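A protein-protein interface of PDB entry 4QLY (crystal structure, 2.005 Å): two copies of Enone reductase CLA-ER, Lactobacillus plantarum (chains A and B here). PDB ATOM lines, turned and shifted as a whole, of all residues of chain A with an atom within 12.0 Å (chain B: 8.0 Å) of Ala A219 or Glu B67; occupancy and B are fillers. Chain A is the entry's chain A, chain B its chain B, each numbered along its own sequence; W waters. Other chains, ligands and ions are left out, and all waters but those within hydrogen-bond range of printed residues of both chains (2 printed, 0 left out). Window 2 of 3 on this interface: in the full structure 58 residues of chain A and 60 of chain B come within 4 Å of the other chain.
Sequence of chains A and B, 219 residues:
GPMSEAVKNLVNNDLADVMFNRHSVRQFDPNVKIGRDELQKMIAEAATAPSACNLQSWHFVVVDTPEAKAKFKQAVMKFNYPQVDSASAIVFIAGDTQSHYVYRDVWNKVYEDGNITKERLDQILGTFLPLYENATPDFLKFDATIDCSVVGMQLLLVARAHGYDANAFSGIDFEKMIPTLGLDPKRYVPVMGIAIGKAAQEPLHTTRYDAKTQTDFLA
The guanidinium group of Arg B36 lies within salt-bridge range of the side-chain carboxylate of Asp B64. OG1 of Thr B65 is in hydrogen-bond range of N of Ala B68 (3.2 Å).
Among the printed residues, pairs that only touch across the chains: Thr A215 with Val B62, Asp A216 with Val B61, Phe A217 with Arg B36, Phe A217 with Val B62, Leu A218 with Val B63, Leu A218 with Ala B68, Ala A219 with Thr B65, Ala A219 with Glu B67 and Ala A219 with Ala B68.
No position is printed for both chains. Of the 12 pairs that touch across the chains among the printed residues, none has its exchanged pair printed and touching as well.
Water W2 lies within hydrogen-bond range of OE1 of Glu B67, OG1 of Thr B65 and O of Ala A219. Water W1 lies within hydrogen-bond range of OD1 of Asp B64, O of Val B62 and N of Ala A219.
Of chain B, only Arg B36 (3.2 Å), Thr B65 (3.4 Å), Glu B67 (3.5 Å) and Ala B68 (3.7 Å) come within 4 Å of Ala A219. Glu B67 touches one residue of chain A. Val B63 touches just one residue of chain A: Leu A218 (3.9 Å). Thr B65 touches just one residue of chain A: Ala A219. Ala B68 touches two residues of chain A. Of the printed residues of chain B, Thr A215 touches Val B62. Printed residues of chain A within 4 Å of Arg B36: Phe A217 (3.3 Å) and Ala A219 (3.2 Å). Printed residues of chain A within 4 Å of Val B61: Asp A216. Of the printed residues of chain A, Val B62 touches Thr A215, Asp A216, Phe A217 and Leu A218. Gln B74 touches none of the printed residues of chain A. The nearest residue of chain A that does not touch Glu B67 is Leu A218 (5.9 Å). The nearest printed residue of chain B that does not touch Asp A216 is Val B63 (5.6 Å).
Of the 15 printed residues of chain B, 7 touch a printed residue of chain A. Hydrophobic or aromatic side chains of chain B within 4 Å of the printed part of chain A: Val B61, Val B62, Val B63 and Ala B68. Of the 5 printed residues of chain A, 5 touch a printed residue of chain B. Among the printed residues, 12 pairs touch across the chains. Among the printed residues, no Asp or Glu carboxylate lies within 4 Å of a Lys or Arg side-chain nitrogen of the other chain.
The backbone carbonyl oxygen (O) of Asp A216 lies within hydrogen-bond range of the backbone NH (N) of Val B62 (2.6 Å). The backbone NH (N) of Leu A218 is in hydrogen-bond range of the backbone carbonyl oxygen (O) of Val B62, at 3.0 Å. The guanidinium group of Arg B36 is in hydrogen-bond range of the backbone carbonyl oxygen of Ala A219.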
ATOM      1  N   THR A 215     -34.468 -14.923  -3.195  1.00  0.00           N
ATOM      2  CA  THR A 215     -33.449 -15.757  -3.827  1.00  0.00           C
ATOM      3  C   THR A 215     -32.865 -15.114  -5.089  1.00  0.00           C
ATOM      4  O   THR A 215     -33.607 -14.713  -5.999  1.00  0.00           O
ATOM      5  CB  THR A 215     -34.040 -17.140  -4.196  1.00  0.00           C
ATOM      6  OG1 THR A 215     -34.625 -17.747  -3.033  1.00  0.00           O
ATOM      7  CG2 THR A 215     -32.976 -18.064  -4.790  1.00  0.00           C
ATOM      8  N   ASP A 216     -31.539 -15.008  -5.136  1.00  0.00           N
ATOM      9  CA  ASP A 216     -30.838 -14.546  -6.337  1.00  0.00           C
ATOM     10  C   ASP A 216     -29.986 -15.660  -6.921  1.00  0.00           C
ATOM     11  O   ASP A 216     -29.384 -16.438  -6.180  1.00  0.00           O
ATOM     12  CB  ASP A 216     -29.943 -13.336  -6.034  1.00  0.00           C
ATOM     13  CG  ASP A 216     -30.714 -12.166  -5.452  1.00  0.00           C
ATOM     14  OD1 ASP A 216     -31.805 -11.840  -5.977  1.00  0.00           O
ATOM     15  OD2 ASP A 216     -30.233 -11.563  -4.473  1.00  0.00           O
ATOM     16  N   PHE A 217     -29.923 -15.737  -8.247  1.00  0.00           N
ATOM     17  CA  PHE A 217     -28.940 -16.599  -8.877  1.00  0.00           C
ATOM     18  C   PHE A 217     -27.792 -15.726  -9.336  1.00  0.00           C
ATOM     19  O   PHE A 217     -27.988 -14.799 -10.124  1.00  0.00           O
ATOM     20  CB  PHE A 217     -29.555 -17.401 -10.023  1.00  0.00           C
ATOM     21  CG  PHE A 217     -30.487 -18.471  -9.550  1.00  0.00           C
ATOM     22  CD1 PHE A 217     -31.815 -18.172  -9.262  1.00  0.00           C
ATOM     23  CD2 PHE A 217     -30.033 -19.762  -9.344  1.00  0.00           C
ATOM     24  CE1 PHE A 217     -32.677 -19.146  -8.793  1.00  0.00           C
ATOM     25  CE2 PHE A 217     -30.889 -20.750  -8.872  1.00  0.00           C
ATOM     26  CZ  PHE A 217     -32.219 -20.436  -8.598  1.00  0.00           C
ATOM     27  N   LEU A 218     -26.609 -15.991  -8.786  1.00  0.00           N
ATOM     28  CA  LEU A 218     -25.420 -15.174  -9.040  1.00  0.00           C
ATOM     29  C   LEU A 218     -25.102 -15.111 -10.529  1.00  0.00           C
ATOM     30  O   LEU A 218     -24.842 -14.039 -11.082  1.00  0.00           O
ATOM     31  CB  LEU A 218     -24.213 -15.724  -8.278  1.00  0.00           C
ATOM     32  CG  LEU A 218     -22.954 -14.857  -8.315  1.00  0.00           C
ATOM     33  CD1 LEU A 218     -23.304 -13.420  -7.944  1.00  0.00           C
ATOM     34  CD2 LEU A 218     -21.874 -15.426  -7.364  1.00  0.00           C
ATOM     35  N   ALA A 219     -25.099 -16.275 -11.164  1.00  0.00           N
ATOM     36  CA  ALA A 219     -25.090 -16.335 -12.613  1.00  0.00           C
ATOM     37  C   ALA A 219     -26.100 -17.394 -13.056  1.00  0.00           C
ATOM     38  O   ALA A 219     -25.810 -18.217 -13.921  1.00  0.00           O
ATOM     39  CB  ALA A 219     -23.678 -16.642 -13.149  1.00  0.00           C
ATOM     40  N   ARG B  36     -32.741 -25.811 -11.183  1.00  0.00           N
ATOM     41  CA  ARG B  36     -33.052 -24.623 -10.399  1.00  0.00           C
ATOM     42  C   ARG B  36     -34.451 -24.679  -9.797  1.00  0.00           C
ATOM     43  O   ARG B  36     -34.735 -23.995  -8.814  1.00  0.00           O
ATOM     44  CB  ARG B  36     -32.890 -23.372 -11.243  1.00  0.00           C
ATOM     45  CG  ARG B  36     -31.455 -23.164 -11.674  1.00  0.00           C
ATOM     46  CD  ARG B  36     -31.229 -21.768 -12.161  1.00  0.00           C
ATOM     47  NE  ARG B  36     -29.811 -21.451 -12.177  1.00  0.00           N
ATOM     48  CZ  ARG B  36     -29.293 -20.450 -12.868  1.00  0.00           C
ATOM     49  NH1 ARG B  36     -27.983 -20.233 -12.824  1.00  0.00           N
ATOM     50  NH2 ARG B  36     -30.094 -19.672 -13.605  1.00  0.00           N
ATOM     51  N   VAL B  61     -28.338 -16.397  -2.063  1.00  0.00           N
ATOM     52  CA  VAL B  61     -27.701 -16.233  -3.373  1.00  0.00           C
ATOM     53  C   VAL B  61     -27.218 -17.600  -3.841  1.00  0.00           C
ATOM     54  O   VAL B  61     -26.397 -18.238  -3.174  1.00  0.00           O
ATOM     55  CB  VAL B  61     -26.536 -15.235  -3.327  1.00  0.00           C
ATOM     56  CG1 VAL B  61     -25.937 -15.054  -4.710  1.00  0.00           C
ATOM     57  CG2 VAL B  61     -27.010 -13.890  -2.767  1.00  0.00           C
ATOM     58  N   VAL B  62     -27.761 -18.074  -4.957  1.00  0.00           N
ATOM     59  CA  VAL B  62     -27.462 -19.425  -5.422  1.00  0.00           C
ATOM     60  C   VAL B  62     -26.319 -19.379  -6.440  1.00  0.00           C
ATOM     61  O   VAL B  62     -26.333 -18.582  -7.380  1.00  0.00           O
ATOM     62  CB  VAL B  62     -28.702 -20.106  -6.029  1.00  0.00           C
ATOM     63  CG1 VAL B  62     -28.366 -21.495  -6.555  1.00  0.00           C
ATOM     64  CG2 VAL B  62     -29.808 -20.215  -4.979  1.00  0.00           C
ATOM     65  N   VAL B  63     -25.326 -20.225  -6.212  1.00  0.00           N
ATOM     66  CA  VAL B  63     -24.119 -20.295  -7.017  1.00  0.00           C
ATOM     67  C   VAL B  63     -24.071 -21.682  -7.629  1.00  0.00           C
ATOM     68  O   VAL B  63     -23.726 -22.658  -6.944  1.00  0.00           O
ATOM     69  CB  VAL B  63     -22.862 -20.051  -6.161  1.00  0.00           C
ATOM     70  CG1 VAL B  63     -21.598 -20.163  -7.017  1.00  0.00           C
ATOM     71  CG2 VAL B  63     -22.951 -18.683  -5.480  1.00  0.00           C
ATOM     72  N   ASP B  64     -24.426 -21.793  -8.904  1.00  0.00           N
ATOM     73  CA  ASP B  64     -24.587 -23.123  -9.479  1.00  0.00           C
ATOM     74  C   ASP B  64     -24.047 -23.233 -10.908  1.00  0.00           C
ATOM     75  O   ASP B  64     -24.394 -24.166 -11.637  1.00  0.00           O
ATOM     76  CB  ASP B  64     -26.059 -23.528  -9.447  1.00  0.00           C
ATOM     77  CG  ASP B  64     -26.938 -22.633 -10.330  1.00  0.00           C
ATOM     78  OD1 ASP B  64     -26.502 -21.514 -10.693  1.00  0.00           O
ATOM     79  OD2 ASP B  64     -28.074 -23.051 -10.643  1.00  0.00           O
ATOM     80  N   THR B  65     -23.213 -22.277 -11.304  1.00  0.00           N
ATOM     81  CA  THR B  65     -22.522 -22.354 -12.596  1.00  0.00           C
ATOM     82  C   THR B  65     -21.019 -22.157 -12.376  1.00  0.00           C
ATOM     83  O   THR B  65     -20.613 -21.631 -11.344  1.00  0.00           O
ATOM     84  CB  THR B  65     -23.054 -21.290 -13.604  1.00  0.00           C
ATOM     85  OG1 THR B  65     -22.703 -19.976 -13.146  1.00  0.00           O
ATOM     86  CG2 THR B  65     -24.571 -21.392 -13.750  1.00  0.00           C
ATOM     87  N   PRO B  66     -20.187 -22.576 -13.343  1.00  0.00           N
ATOM     88  CA  PRO B  66     -18.746 -22.346 -13.189  1.00  0.00           C
ATOM     89  C   PRO B  66     -18.400 -20.868 -13.060  1.00  0.00           C
ATOM     90  O   PRO B  66     -17.625 -20.495 -12.179  1.00  0.00           O
ATOM     91  CB  PRO B  66     -18.161 -22.946 -14.471  1.00  0.00           C
ATOM     92  CG  PRO B  66     -19.105 -24.052 -14.798  1.00  0.00           C
ATOM     93  CD  PRO B  66     -20.476 -23.518 -14.440  1.00  0.00           C
ATOM     94  N   GLU B  67     -18.983 -20.036 -13.918  1.00  0.00           N
ATOM     95  CA  GLU B  67     -18.779 -18.591 -13.845  1.00  0.00           C
ATOM     96  C   GLU B  67     -19.102 -18.032 -12.471  1.00  0.00           C
ATOM     97  O   GLU B  67     -18.354 -17.206 -11.937  1.00  0.00           O
ATOM     98  CB  GLU B  67     -19.643 -17.859 -14.883  1.00  0.00           C
ATOM     99  CG  GLU B  67     -19.866 -16.380 -14.539  1.00  0.00           C
ATOM    100  CD  GLU B  67     -20.920 -15.700 -15.414  1.00  0.00           C
ATOM    101  OE1 GLU B  67     -21.744 -16.407 -16.037  1.00  0.00           O
ATOM    102  OE2 GLU B  67     -20.921 -14.452 -15.474  1.00  0.00           O
ATOM    103  N   ALA B  68     -20.230 -18.463 -11.908  1.00  0.00           N
ATOM    104  CA  ALA B  68     -20.644 -17.971 -10.606  1.00  0.00           C
ATOM    105  C   ALA B  68     -19.688 -18.484  -9.522  1.00  0.00           C
ATOM    106  O   ALA B  68     -19.361 -17.760  -8.591  1.00  0.00           O
ATOM    107  CB  ALA B  68     -22.082 -18.380 -10.296  1.00  0.00           C
ATOM    108  N   LYS B  69     -19.233 -19.723  -9.659  1.00  0.00           N
ATOM    109  CA  LYS B  69     -18.297 -20.284  -8.681  1.00  0.00           C
ATOM    110  C   LYS B  69     -16.983 -19.503  -8.651  1.00  0.00           C
ATOM    111  O   LYS B  69     -16.494 -19.151  -7.583  1.00  0.00           O
ATOM    112  CB  LYS B  69     -18.021 -21.757  -8.973  1.00  0.00           C
ATOM    113  CG  LYS B  69     -19.144 -22.690  -8.571  1.00  0.00           C
ATOM    114  CD  LYS B  69     -18.722 -24.131  -8.760  1.00  0.00           C
ATOM    115  CE  LYS B  69     -19.855 -25.098  -8.495  1.00  0.00           C
ATOM    116  NZ  LYS B  69     -19.420 -26.510  -8.705  1.00  0.00           N
ATOM    117  N   ALA B  70     -16.419 -19.224  -9.826  1.00  0.00           N
ATOM    118  CA  ALA B  70     -15.167 -18.474  -9.910  1.00  0.00           C
ATOM    119  C   ALA B  70     -15.275 -17.088  -9.267  1.00  0.00           C
ATOM    120  O   ALA B  70     -14.343 -16.629  -8.619  1.00  0.00           O
ATOM    121  CB  ALA B  70     -14.711 -18.347 -11.379  1.00  0.00           C
ATOM    122  N   LYS B  71     -16.403 -16.410  -9.437  1.00  0.00           N
ATOM    123  CA  LYS B  71     -16.566 -15.119  -8.776  1.00  0.00           C
ATOM    124  C   LYS B  71     -16.739 -15.280  -7.250  1.00  0.00           C
ATOM    125  O   LYS B  71     -16.099 -14.582  -6.456  1.00  0.00           O
ATOM    126  CB  LYS B  71     -17.749 -14.365  -9.378  1.00  0.00           C
ATOM    127  CG  LYS B  71     -18.256 -13.228  -8.511  1.00  0.00           C
ATOM    128  CD  LYS B  71     -19.040 -12.205  -9.324  1.00  0.00           C
ATOM    129  CE  LYS B  71     -18.623 -12.205 -10.795  1.00  0.00           C
ATOM    130  NZ  LYS B  71     -19.170 -11.021 -11.514  1.00  0.00           N
ATOM    131  N   PHE B  72     -17.597 -16.212  -6.861  1.00  0.00           N
ATOM    132  CA  PHE B  72     -17.905 -16.494  -5.455  1.00  0.00           C
ATOM    133  C   PHE B  72     -16.636 -16.851  -4.661  1.00  0.00           C
ATOM    134  O   PHE B  72     -16.427 -16.347  -3.552  1.00  0.00           O
ATOM    135  CB  PHE B  72     -18.953 -17.622  -5.402  1.00  0.00           C
ATOM    136  CG  PHE B  72     -19.324 -18.084  -4.014  1.00  0.00           C
ATOM    137  CD1 PHE B  72     -19.963 -17.235  -3.131  1.00  0.00           C
ATOM    138  CD2 PHE B  72     -19.086 -19.395  -3.627  1.00  0.00           C
ATOM    139  CE1 PHE B  72     -20.324 -17.674  -1.864  1.00  0.00           C
ATOM    140  CE2 PHE B  72     -19.435 -19.845  -2.359  1.00  0.00           C
ATOM    141  CZ  PHE B  72     -20.061 -18.979  -1.479  1.00  0.00           C
ATOM    142  N   LYS B  73     -15.781 -17.685  -5.253  1.00  0.00           N
ATOM    143  CA  LYS B  73     -14.563 -18.174  -4.596  1.00  0.00           C
ATOM    144  C   LYS B  73     -13.607 -17.051  -4.208  1.00  0.00           C
ATOM    145  O   LYS B  73     -12.781 -17.227  -3.330  1.00  0.00           O
ATOM    146  CB  LYS B  73     -13.832 -19.167  -5.494  1.00  0.00           C
ATOM    147  CG  LYS B  73     -14.430 -20.548  -5.515  1.00  0.00           C
ATOM    148  CD  LYS B  73     -13.802 -21.422  -6.605  1.00  0.00           C
ATOM    149  CE  LYS B  73     -12.396 -21.887  -6.262  1.00  0.00           C
ATOM    150  NZ  LYS B  73     -11.902 -22.879  -7.272  1.00  0.00           N
ATOM    151  N   GLN B  74     -13.726 -15.896  -4.853  1.00  0.00           N
ATOM    152  CA  GLN B  74     -12.899 -14.743  -4.496  1.00  0.00           C
ATOM    153  C   GLN B  74     -13.139 -14.280  -3.060  1.00  0.00           C
ATOM    154  O   GLN B  74     -12.317 -13.563  -2.480  1.00  0.00           O
ATOM    155  CB  GLN B  74     -13.161 -13.573  -5.459  1.00  0.00           C
ATOM    156  CG  GLN B  74     -12.775 -13.867  -6.903  1.00  0.00           C
ATOM    157  CD  GLN B  74     -13.256 -12.795  -7.877  1.00  0.00           C
ATOM    158  OE1 GLN B  74     -14.099 -11.948  -7.543  1.00  0.00           O
ATOM    159  NE2 GLN B  74     -12.718 -12.831  -9.093  1.00  0.00           N
HETATM  160  O   HOH W   1     -25.443 -19.192 -10.008  1.00  0.00           O
HETATM  161  O   HOH W   2     -23.281 -18.496 -15.872  1.00  0.00           O
